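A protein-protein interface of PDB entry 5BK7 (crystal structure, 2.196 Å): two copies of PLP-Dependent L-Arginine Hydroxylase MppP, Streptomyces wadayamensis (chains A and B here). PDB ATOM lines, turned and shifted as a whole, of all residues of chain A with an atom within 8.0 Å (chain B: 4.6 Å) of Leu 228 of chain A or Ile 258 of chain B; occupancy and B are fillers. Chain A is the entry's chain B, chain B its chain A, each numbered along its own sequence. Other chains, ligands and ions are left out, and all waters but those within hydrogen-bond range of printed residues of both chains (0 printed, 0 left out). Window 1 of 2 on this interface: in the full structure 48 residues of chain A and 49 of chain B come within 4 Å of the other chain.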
ATOM      1  N   VAL A  42      -2.632  24.120  21.343  1.00  0.00           N
ATOM      2  CA  VAL A  42      -1.896  23.014  21.944  1.00  0.00           C
ATOM      3  C   VAL A  42      -1.985  23.095  23.452  1.00  0.00           C
ATOM      4  O   VAL A  42      -1.942  22.069  24.146  1.00  0.00           O
ATOM      5  CB  VAL A  42      -0.424  23.017  21.493  1.00  0.00           C
ATOM      6  CG1 VAL A  42       0.476  22.171  22.439  1.00  0.00           C
ATOM      7  CG2 VAL A  42      -0.308  22.505  20.075  1.00  0.00           C
ATOM      8  N   LEU A  45      -4.931  21.328  25.191  1.00  0.00           N
ATOM      9  CA  LEU A  45      -5.201  19.930  24.849  1.00  0.00           C
ATOM     10  C   LEU A  45      -5.810  19.147  26.014  1.00  0.00           C
ATOM     11  O   LEU A  45      -6.741  18.356  25.756  1.00  0.00           O
ATOM     12  CB  LEU A  45      -3.931  19.221  24.330  1.00  0.00           C
ATOM     13  CG  LEU A  45      -3.707  19.334  22.831  1.00  0.00           C
ATOM     14  CD1 LEU A  45      -2.312  18.873  22.475  1.00  0.00           C
ATOM     15  CD2 LEU A  45      -4.719  18.539  22.060  1.00  0.00           C
ATOM     16  N   TYR A  88      -8.443   8.218   8.508  1.00  0.00           N
ATOM     17  CA  TYR A  88      -7.169   8.518   9.148  1.00  0.00           C
ATOM     18  C   TYR A  88      -6.344   9.488   8.316  1.00  0.00           C
ATOM     19  O   TYR A  88      -5.572  10.291   8.858  1.00  0.00           O
ATOM     20  CB  TYR A  88      -6.380   7.208   9.393  1.00  0.00           C
ATOM     21  CG  TYR A  88      -7.087   6.261  10.344  1.00  0.00           C
ATOM     22  CD1 TYR A  88      -7.418   6.657  11.648  1.00  0.00           C
ATOM     23  CD2 TYR A  88      -7.439   4.988   9.940  1.00  0.00           C
ATOM     24  CE1 TYR A  88      -8.070   5.809  12.509  1.00  0.00           C
ATOM     25  CE2 TYR A  88      -8.106   4.131  10.796  1.00  0.00           C
ATOM     26  CZ  TYR A  88      -8.430   4.540  12.073  1.00  0.00           C
ATOM     27  OH  TYR A  88      -9.099   3.650  12.897  1.00  0.00           O
ATOM     28  N   ASP A 218      -8.494  17.056   2.702  1.00  0.00           N
ATOM     29  CA  ASP A 218      -7.371  16.719   3.571  1.00  0.00           C
ATOM     30  C   ASP A 218      -7.079  17.930   4.444  1.00  0.00           C
ATOM     31  O   ASP A 218      -7.001  19.033   3.928  1.00  0.00           O
ATOM     32  CB  ASP A 218      -6.131  16.328   2.742  1.00  0.00           C
ATOM     33  CG  ASP A 218      -4.928  15.878   3.603  1.00  0.00           C
ATOM     34  OD1 ASP A 218      -5.032  15.764   4.857  1.00  0.00           O
ATOM     35  OD2 ASP A 218      -3.856  15.624   3.011  1.00  0.00           O
ATOM     36  N   THR A 219      -6.936  17.737   5.754  1.00  0.00           N
ATOM     37  CA  THR A 219      -6.511  18.792   6.674  1.00  0.00           C
ATOM     38  C   THR A 219      -5.011  18.754   7.005  1.00  0.00           C
ATOM     39  O   THR A 219      -4.510  19.658   7.673  1.00  0.00           O
ATOM     40  CB  THR A 219      -7.345  18.714   7.964  1.00  0.00           C
ATOM     41  OG1 THR A 219      -6.921  17.616   8.774  1.00  0.00           O
ATOM     42  CG2 THR A 219      -8.818  18.515   7.665  1.00  0.00           C
ATOM     43  N   GLY A 220      -4.272  17.785   6.475  1.00  0.00           N
ATOM     44  CA  GLY A 220      -2.903  17.566   6.913  1.00  0.00           C
ATOM     45  C   GLY A 220      -1.912  18.625   6.468  1.00  0.00           C
ATOM     46  O   GLY A 220      -1.103  19.083   7.268  1.00  0.00           O
ATOM     47  N   TRP A 223      -1.513  22.744   8.376  1.00  0.00           N
ATOM     48  CA  TRP A 223      -1.022  23.228   9.658  1.00  0.00           C
ATOM     49  C   TRP A 223      -0.056  22.237  10.290  1.00  0.00           C
ATOM     50  O   TRP A 223      -0.175  21.027  10.071  1.00  0.00           O
ATOM     51  CB  TRP A 223      -2.179  23.473  10.623  1.00  0.00           C
ATOM     52  CG  TRP A 223      -3.248  24.304  10.068  1.00  0.00           C
ATOM     53  CD1 TRP A 223      -3.142  25.595   9.614  1.00  0.00           C
ATOM     54  CD2 TRP A 223      -4.620  23.935   9.917  1.00  0.00           C
ATOM     55  NE1 TRP A 223      -4.366  26.033   9.170  1.00  0.00           N
ATOM     56  CE2 TRP A 223      -5.291  25.036   9.355  1.00  0.00           C
ATOM     57  CE3 TRP A 223      -5.339  22.789  10.203  1.00  0.00           C
ATOM     58  CZ2 TRP A 223      -6.655  25.016   9.074  1.00  0.00           C
ATOM     59  CZ3 TRP A 223      -6.701  22.774   9.917  1.00  0.00           C
ATOM     60  CH2 TRP A 223      -7.335  23.871   9.356  1.00  0.00           C
ATOM     61  N   PRO A 224       0.919  22.728  11.105  1.00  0.00           N
ATOM     62  CA  PRO A 224       1.887  21.835  11.754  1.00  0.00           C
ATOM     63  C   PRO A 224       1.319  21.135  12.990  1.00  0.00           C
ATOM     64  O   PRO A 224       1.598  21.461  14.153  1.00  0.00           O
ATOM     65  CB  PRO A 224       3.036  22.781  12.102  1.00  0.00           C
ATOM     66  CG  PRO A 224       2.448  24.171  12.098  1.00  0.00           C
ATOM     67  CD  PRO A 224       1.058  24.111  11.595  1.00  0.00           C
ATOM     68  N   THR A 225       0.520  20.108  12.704  1.00  0.00           N
ATOM     69  CA  THR A 225      -0.218  19.310  13.675  1.00  0.00           C
ATOM     70  C   THR A 225       0.422  17.945  13.935  1.00  0.00           C
ATOM     71  O   THR A 225      -0.253  17.049  14.449  1.00  0.00           O
ATOM     72  CB  THR A 225      -1.630  19.062  13.175  1.00  0.00           C
ATOM     73  OG1 THR A 225      -1.529  18.377  11.914  1.00  0.00           O
ATOM     74  CG2 THR A 225      -2.433  20.377  13.052  1.00  0.00           C
ATOM     75  N   LEU A 226       1.683  17.755  13.569  1.00  0.00           N
ATOM     76  CA  LEU A 226       2.370  16.522  13.887  1.00  0.00           C
ATOM     77  C   LEU A 226       1.656  15.329  13.258  1.00  0.00           C
ATOM     78  O   LEU A 226       1.609  14.230  13.825  1.00  0.00           O
ATOM     79  CB  LEU A 226       2.481  16.357  15.413  1.00  0.00           C
ATOM     80  CG  LEU A 226       3.213  17.452  16.194  1.00  0.00           C
ATOM     81  CD1 LEU A 226       3.124  17.203  17.687  1.00  0.00           C
ATOM     82  CD2 LEU A 226       4.677  17.555  15.808  1.00  0.00           C
ATOM     83  N   ASP A 227       1.092  15.538  12.070  1.00  0.00           N
ATOM     84  CA  ASP A 227       0.429  14.487  11.289  1.00  0.00           C
ATOM     85  C   ASP A 227      -0.868  13.998  11.929  1.00  0.00           C
ATOM     86  O   ASP A 227      -1.349  12.913  11.598  1.00  0.00           O
ATOM     87  CB  ASP A 227       1.362  13.295  11.013  1.00  0.00           C
ATOM     88  CG  ASP A 227       1.884  13.283   9.588  1.00  0.00           C
ATOM     89  OD1 ASP A 227       1.052  13.256   8.649  1.00  0.00           O
ATOM     90  OD2 ASP A 227       3.130  13.329   9.408  1.00  0.00           O
ATOM     91  N   LEU A 228      -1.452  14.807  12.810  1.00  0.00           N
ATOM     92  CA  LEU A 228      -2.799  14.605  13.344  1.00  0.00           C
ATOM     93  C   LEU A 228      -3.798  15.286  12.420  1.00  0.00           C
ATOM     94  O   LEU A 228      -3.769  16.506  12.289  1.00  0.00           O
ATOM     95  CB  LEU A 228      -2.903  15.216  14.738  1.00  0.00           C
ATOM     96  CG  LEU A 228      -1.921  14.647  15.754  1.00  0.00           C
ATOM     97  CD1 LEU A 228      -1.843  15.539  16.991  1.00  0.00           C
ATOM     98  CD2 LEU A 228      -2.353  13.227  16.100  1.00  0.00           C
ATOM     99  N   LYS A 229      -4.678  14.518  11.796  1.00  0.00           N
ATOM    100  CA  LYS A 229      -5.347  14.983  10.587  1.00  0.00           C
ATOM    101  C   LYS A 229      -6.481  14.034  10.256  1.00  0.00           C
ATOM    102  O   LYS A 229      -6.610  12.960  10.850  1.00  0.00           O
ATOM    103  CB  LYS A 229      -4.381  15.005   9.411  1.00  0.00           C
ATOM    104  CG  LYS A 229      -3.982  13.589   8.989  1.00  0.00           C
ATOM    105  CD  LYS A 229      -2.571  13.494   8.405  1.00  0.00           C
ATOM    106  CE  LYS A 229      -2.269  12.078   7.987  1.00  0.00           C
ATOM    107  NZ  LYS A 229      -0.996  12.031   7.268  1.00  0.00           N
ATOM    108  N   ALA A 230      -7.249  14.403   9.240  1.00  0.00           N
ATOM    109  CA  ALA A 230      -8.237  13.518   8.652  1.00  0.00           C
ATOM    110  C   ALA A 230      -8.285  13.734   7.143  1.00  0.00           C
ATOM    111  O   ALA A 230      -8.022  14.829   6.643  1.00  0.00           O
ATOM    112  CB  ALA A 230      -9.636  13.735   9.232  1.00  0.00           C
ATOM    113  N   SER A 255     -10.472   9.750  15.637  1.00  0.00           N
ATOM    114  CA  SER A 255     -10.384  10.129  17.042  1.00  0.00           C
ATOM    115  C   SER A 255     -11.152  11.424  17.264  1.00  0.00           C
ATOM    116  O   SER A 255     -10.882  12.426  16.577  1.00  0.00           O
ATOM    117  CB  SER A 255      -8.923  10.330  17.473  1.00  0.00           C
ATOM    118  OG  SER A 255      -8.836  11.169  18.646  1.00  0.00           O
ATOM    119  N   LEU A 257     -10.609  13.519  19.364  1.00  0.00           N
ATOM    120  CA  LEU A 257      -9.687  14.585  19.706  1.00  0.00           C
ATOM    121  C   LEU A 257      -9.098  15.215  18.452  1.00  0.00           C
ATOM    122  O   LEU A 257      -8.931  16.443  18.399  1.00  0.00           O
ATOM    123  CB  LEU A 257      -8.579  14.081  20.623  1.00  0.00           C
ATOM    124  CG  LEU A 257      -7.661  15.190  21.147  1.00  0.00           C
ATOM    125  CD1 LEU A 257      -8.391  16.032  22.168  1.00  0.00           C
ATOM    126  CD2 LEU A 257      -6.407  14.570  21.732  1.00  0.00           C
ATOM    127  N   ILE A 258      -8.752  14.392  17.446  1.00  0.00           N
ATOM    128  CA  ILE A 258      -8.259  14.912  16.184  1.00  0.00           C
ATOM    129  C   ILE A 258      -9.308  15.807  15.540  1.00  0.00           C
ATOM    130  O   ILE A 258      -8.995  16.853  14.946  1.00  0.00           O
ATOM    131  CB  ILE A 258      -7.857  13.759  15.240  1.00  0.00           C
ATOM    132  CG1 ILE A 258      -6.589  13.065  15.737  1.00  0.00           C
ATOM    133  CG2 ILE A 258      -7.598  14.278  13.827  1.00  0.00           C
ATOM    134  CD1 ILE A 258      -6.019  12.021  14.799  1.00  0.00           C
ATOM    135  N   LEU A 259     -10.565  15.392  15.621  1.00  0.00           N
ATOM    136  CA  LEU A 259     -11.649  16.198  15.080  1.00  0.00           C
ATOM    137  C   LEU A 259     -11.754  17.537  15.817  1.00  0.00           C
ATOM    138  O   LEU A 259     -11.929  18.588  15.196  1.00  0.00           O
ATOM    139  CB  LEU A 259     -12.958  15.429  15.198  1.00  0.00           C
ATOM    140  CG  LEU A 259     -13.741  14.714  14.069  1.00  0.00           C
ATOM    141  CD1 LEU A 259     -13.254  14.931  12.645  1.00  0.00           C
ATOM    142  CD2 LEU A 259     -13.907  13.269  14.347  1.00  0.00           C
ATOM    143  N   LEU A 261      -9.458  19.100  17.238  1.00  0.00           N
ATOM    144  CA  LEU A 261      -8.279  19.875  16.884  1.00  0.00           C
ATOM    145  C   LEU A 261      -8.416  20.501  15.501  1.00  0.00           C
ATOM    146  O   LEU A 261      -7.901  21.608  15.260  1.00  0.00           O
ATOM    147  CB  LEU A 261      -7.073  18.961  16.921  1.00  0.00           C
ATOM    148  CG  LEU A 261      -5.839  19.408  17.643  1.00  0.00           C
ATOM    149  CD1 LEU A 261      -6.112  19.975  19.000  1.00  0.00           C
ATOM    150  CD2 LEU A 261      -5.060  18.171  17.772  1.00  0.00           C
ATOM    151  N   ILE A 262      -9.020  19.756  14.564  1.00  0.00           N
ATOM    152  CA  ILE A 262      -9.338  20.296  13.251  1.00  0.00           C
ATOM    153  C   ILE A 262     -10.245  21.508  13.415  1.00  0.00           C
ATOM    154  O   ILE A 262      -9.998  22.570  12.843  1.00  0.00           O
ATOM    155  CB  ILE A 262     -10.002  19.212  12.374  1.00  0.00           C
ATOM    156  CG1 ILE A 262      -8.982  18.164  12.001  1.00  0.00           C
ATOM    157  CG2 ILE A 262     -10.645  19.845  11.112  1.00  0.00           C
ATOM    158  CD1 ILE A 262      -9.542  17.063  11.108  1.00  0.00           C
ATOM    159  N   PHE A 265      -8.231  24.442  14.997  1.00  0.00           N
ATOM    160  CA  PHE A 265      -7.290  25.020  14.037  1.00  0.00           C
ATOM    161  C   PHE A 265      -8.020  25.701  12.868  1.00  0.00           C
ATOM    162  O   PHE A 265      -7.535  26.705  12.328  1.00  0.00           O
ATOM    163  CB  PHE A 265      -6.343  23.955  13.470  1.00  0.00           C
ATOM    164  CG  PHE A 265      -5.106  23.734  14.284  1.00  0.00           C
ATOM    165  CD1 PHE A 265      -5.173  23.118  15.522  1.00  0.00           C
ATOM    166  CD2 PHE A 265      -3.877  24.112  13.812  1.00  0.00           C
ATOM    167  CE1 PHE A 265      -4.028  22.903  16.270  1.00  0.00           C
ATOM    168  CE2 PHE A 265      -2.717  23.900  14.548  1.00  0.00           C
ATOM    169  CZ  PHE A 265      -2.795  23.286  15.772  1.00  0.00           C
ATOM    170  N   TRP B  49       3.901  17.341  23.106  1.00  0.00           N
ATOM    171  CA  TRP B  49       3.801  17.979  21.788  1.00  0.00           C
ATOM    172  C   TRP B  49       5.125  18.643  21.428  1.00  0.00           C
ATOM    173  O   TRP B  49       5.666  18.448  20.332  1.00  0.00           O
ATOM    174  CB  TRP B  49       2.662  19.014  21.781  1.00  0.00           C
ATOM    175  CG  TRP B  49       2.448  19.587  20.407  1.00  0.00           C
ATOM    176  CD1 TRP B  49       3.332  20.374  19.681  1.00  0.00           C
ATOM    177  CD2 TRP B  49       1.294  19.413  19.572  1.00  0.00           C
ATOM    178  NE1 TRP B  49       2.791  20.673  18.458  1.00  0.00           N
ATOM    179  CE2 TRP B  49       1.539  20.121  18.368  1.00  0.00           C
ATOM    180  CE3 TRP B  49       0.070  18.731  19.724  1.00  0.00           C
ATOM    181  CZ2 TRP B  49       0.614  20.159  17.327  1.00  0.00           C
ATOM    182  CZ3 TRP B  49      -0.848  18.789  18.701  1.00  0.00           C
ATOM    183  CH2 TRP B  49      -0.574  19.492  17.510  1.00  0.00           C
ATOM    184  N   LEU B 228      -6.492   7.171  19.732  1.00  0.00           N
ATOM    185  CA  LEU B 228      -5.130   7.525  19.332  1.00  0.00           C
ATOM    186  C   LEU B 228      -4.266   6.297  19.541  1.00  0.00           C
ATOM    187  O   LEU B 228      -4.042   5.863  20.684  1.00  0.00           O
ATOM    188  CB  LEU B 228      -4.608   8.720  20.133  1.00  0.00           C
ATOM    189  CG  LEU B 228      -5.452  10.010  20.021  1.00  0.00           C
ATOM    190  CD1 LEU B 228      -4.977  11.108  20.998  1.00  0.00           C
ATOM    191  CD2 LEU B 228      -5.454  10.566  18.609  1.00  0.00           C
ATOM    192  N   LYS B 229      -3.839   5.692  18.438  1.00  0.00           N
ATOM    193  CA  LYS B 229      -3.315   4.333  18.512  1.00  0.00           C
ATOM    194  C   LYS B 229      -2.410   4.070  17.321  1.00  0.00           C
ATOM    195  O   LYS B 229      -2.271   4.892  16.403  1.00  0.00           O
ATOM    196  CB  LYS B 229      -4.479   3.338  18.516  1.00  0.00           C
ATOM    197  CG  LYS B 229      -5.153   3.300  17.126  1.00  0.00           C
ATOM    198  CD  LYS B 229      -6.636   2.913  17.219  1.00  0.00           C
ATOM    199  CE  LYS B 229      -7.343   3.113  15.900  1.00  0.00           C
ATOM    200  NZ  LYS B 229      -8.763   2.757  16.053  1.00  0.00           N
ATOM    201  N   SER B 255       1.765   9.915  13.501  1.00  0.00           N
ATOM    202  CA  SER B 255       2.080  11.063  14.330  1.00  0.00           C
ATOM    203  C   SER B 255       3.134  10.718  15.378  1.00  0.00           C
ATOM    204  O   SER B 255       2.983   9.702  16.097  1.00  0.00           O
ATOM    205  CB  SER B 255       0.843  11.577  15.063  1.00  0.00           C
ATOM    206  OG  SER B 255       1.277  12.633  15.867  1.00  0.00           O
ATOM    207  N   PRO B 256       4.189  11.539  15.525  1.00  0.00           N
ATOM    208  CA  PRO B 256       5.127  11.334  16.649  1.00  0.00           C
ATOM    209  C   PRO B 256       4.490  11.566  18.006  1.00  0.00           C
ATOM    210  O   PRO B 256       4.985  11.060  19.029  1.00  0.00           O
ATOM    211  CB  PRO B 256       6.240  12.367  16.373  1.00  0.00           C
ATOM    212  CG  PRO B 256       5.652  13.371  15.507  1.00  0.00           C
ATOM    213  CD  PRO B 256       4.663  12.610  14.621  1.00  0.00           C
ATOM    214  N   LEU B 257       3.435  12.368  18.050  1.00  0.00           N
ATOM    215  CA  LEU B 257       2.693  12.510  19.275  1.00  0.00           C
ATOM    216  C   LEU B 257       2.025  11.203  19.640  1.00  0.00           C
ATOM    217  O   LEU B 257       2.052  10.792  20.803  1.00  0.00           O
ATOM    218  CB  LEU B 257       1.648  13.607  19.147  1.00  0.00           C
ATOM    219  CG  LEU B 257       0.937  13.930  20.465  1.00  0.00           C
ATOM    220  CD1 LEU B 257       1.943  14.379  21.519  1.00  0.00           C
ATOM    221  CD2 LEU B 257      -0.117  15.016  20.311  1.00  0.00           C
ATOM    222  N   ILE B 258       1.387  10.547  18.672  1.00  0.00           N
ATOM    223  CA  ILE B 258       0.733   9.276  18.992  1.00  0.00           C
ATOM    224  C   ILE B 258       1.785   8.299  19.483  1.00  0.00           C
ATOM    225  O   ILE B 258       1.589   7.617  20.487  1.00  0.00           O
ATOM    226  CB  ILE B 258      -0.068   8.743  17.773  1.00  0.00           C
ATOM    227  CG1 ILE B 258      -1.302   9.639  17.538  1.00  0.00           C
ATOM    228  CG2 ILE B 258      -0.599   7.321  17.983  1.00  0.00           C
ATOM    229  CD1 ILE B 258      -2.136   9.271  16.251  1.00  0.00           C
ATOM    230  N   LEU B 259       2.961   8.309  18.851  1.00  0.00           N
ATOM    231  CA  LEU B 259       4.033   7.409  19.254  1.00  0.00           C
ATOM    232  C   LEU B 259       4.551   7.743  20.657  1.00  0.00           C
ATOM    233  O   LEU B 259       4.870   6.844  21.443  1.00  0.00           O
ATOM    234  CB  LEU B 259       5.170   7.496  18.247  1.00  0.00           C
ATOM    235  CG  LEU B 259       5.498   6.451  17.198  1.00  0.00           C
ATOM    236  CD1 LEU B 259       4.323   5.656  16.889  1.00  0.00           C
ATOM    237  CD2 LEU B 259       6.042   7.157  15.928  1.00  0.00           C
ATOM    238  N   ALA B 260       4.666   9.032  20.985  1.00  0.00           N
ATOM    239  CA  ALA B 260       4.962   9.415  22.363  1.00  0.00           C
ATOM    240  C   ALA B 260       3.899   8.889  23.335  1.00  0.00           C
ATOM    241  O   ALA B 260       4.230   8.375  24.418  1.00  0.00           O
ATOM    242  CB  ALA B 260       5.083  10.952  22.441  1.00  0.00           C
ATOM    243  N   LEU B 261       2.608   9.044  22.979  1.00  0.00           N
ATOM    244  CA  LEU B 261       1.521   8.621  23.865  1.00  0.00           C
ATOM    245  C   LEU B 261       1.620   7.137  24.144  1.00  0.00           C
ATOM    246  O   LEU B 261       1.449   6.689  25.287  1.00  0.00           O
ATOM    247  CB  LEU B 261       0.164   8.951  23.227  1.00  0.00           C
ATOM    248  CG  LEU B 261      -0.771  10.031  23.777  1.00  0.00           C
ATOM    249  CD1 LEU B 261      -0.061  10.929  24.725  1.00  0.00           C
ATOM    250  CD2 LEU B 261      -1.425  10.890  22.721  1.00  0.00           C
ATOM    251  N   ILE B 262       1.893   6.356  23.102  1.00  0.00           N
ATOM    252  CA  ILE B 262       2.037   4.932  23.272  1.00  0.00           C
ATOM    253  C   ILE B 262       3.144   4.643  24.258  1.00  0.00           C
ATOM    254  O   ILE B 262       3.012   3.781  25.147  1.00  0.00           O
ATOM    255  CB  ILE B 262       2.287   4.262  21.912  1.00  0.00           C
ATOM    256  CG1 ILE B 262       0.996   4.293  21.060  1.00  0.00           C
ATOM    257  CG2 ILE B 262       2.745   2.812  22.124  1.00  0.00           C
ATOM    258  CD1 ILE B 262       1.236   3.905  19.587  1.00  0.00           C
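Of the 21 printed residues of chain A, 10 touch a printed residue of chain B.
Of the 11 printed residues of chain B, 7 touch a printed residue of chain A.
Hydrophobic or aromatic side chains of chain B within 4 Å of the printed part of chain A: Trp 49, Leu 228, Pro 256, Leu 257 and Ile 258.
Among the printed residues, no Asp or Glu carboxylate lies within 4 Å of a Lys or Arg side-chain nitrogen of the other chain.
Of the printed residues of chain B, Val 42 of chain A touches Trp 49.
Of chain B, only Trp 49, Ser 255, Leu 257 and Ile 258 come within 4 Å of Leu 228 of chain A.
Of the printed residues of chain A, Trp 49 of chain B touches Val 42, Leu 45, Pro 224, Thr 225, Leu 226 and Leu 228.
Printed residues of chain A within 4 Å of Leu 228 of chain B: Ser 255, Leu 257 and Ile 258.
Of the printed residues of chain A, Leu 257 of chain B touches Leu 228 (3.8 Å).
Ile 258 of chain B touches one residue of chain A.
The nearest printed residue of chain B that does not touch Leu 228 of chain A is Leu 228 of chain B (4.8 Å).
The nearest printed residue of chain B that does not touch Ile 258 of chain A is Ile 258 of chain B (5.0 Å).
The backbone NH (N) of Ile 258 of chain B lies within hydrogen-bond range of the side-chain hydroxyl (OG) of Ser 255 of chain B, 3.5 Å away.
The side-chain hydroxyl of Ser 255 of chain B sits at hydrogen-bond distance from the backbone NH of Leu 257 of chain B (3.1 Å).
The backbone NH (N) of Leu 257 of chain A sits close to the side-chain hydroxyl (OG) of Ser 255 of chain A (3.0 Å).
The side-chain hydroxyl of Ser 255 of chain A is in hydrogen-bond range of the backbone NH of Ile 258 of chain A (3.4 Å).
The backbone carbonyl oxygen of Leu 228 of chain A lies within hydrogen-bond range of the side-chain hydroxyl of Thr 225 of chain A (2.9 Å).
The side-chain hydroxyl (OH) of Tyr 88 of chain A is in hydrogen-bond range of the side-chain amino group (NZ) of Lys 229 of chain B (3.3 Å).
The side-chain hydroxyl (OG) of Ser 255 of chain B is in hydrogen-bond range of the backbone carbonyl oxygen (O) of Leu 226 of chain A.
Leu 228 of chain A touches Ser 255 of chain B, and with the chains exchanged Ser 255 of chain A touches Leu 228 of chain B.
Leu 228 of chain A touches Leu 257 of chain B, and with the chains exchanged Leu 257 of chain A touches Leu 228 of chain B.
Leu 228 of chain A touches Ile 258 of chain B, and with the chains exchanged Ile 258 of chain A touches Leu 228 of chain B.
Of the 15 pairs that touch across the chains among the printed residues, 6 have their exchanged pair printed and touching as well.
CE2 of Trp 49 of chain B touches CG2 of Val 42 of chain A, 3.5 Å away.
CE3 of Trp 49 of chain B touches CD1 of Leu 45 of chain A, at 3.6 Å.
Trp 49 of chain B touches Pro 224 of chain A (CZ2 to O, 3.6 Å).
Thr 225 of chain A touches Trp 49 of chain B.
O of Leu 226 of chain A touches CD of Pro 256 of chain B, 3.5 Å away.
CZ3 of Trp 49 of chain B touches CD1 of Leu 228 of chain A (3.8 Å).
OG of Ser 255 of chain B touches CD2 of Leu 228 of chain A, 3.7 Å away.
Ser 255 of chain A touches Leu 228 of chain B.
CD2 of Leu 257 of chain A touches CD1 of Leu 228 of chain B, at 3.8 Å.
Ile 258 of chain A touches Leu 228 of chain B.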
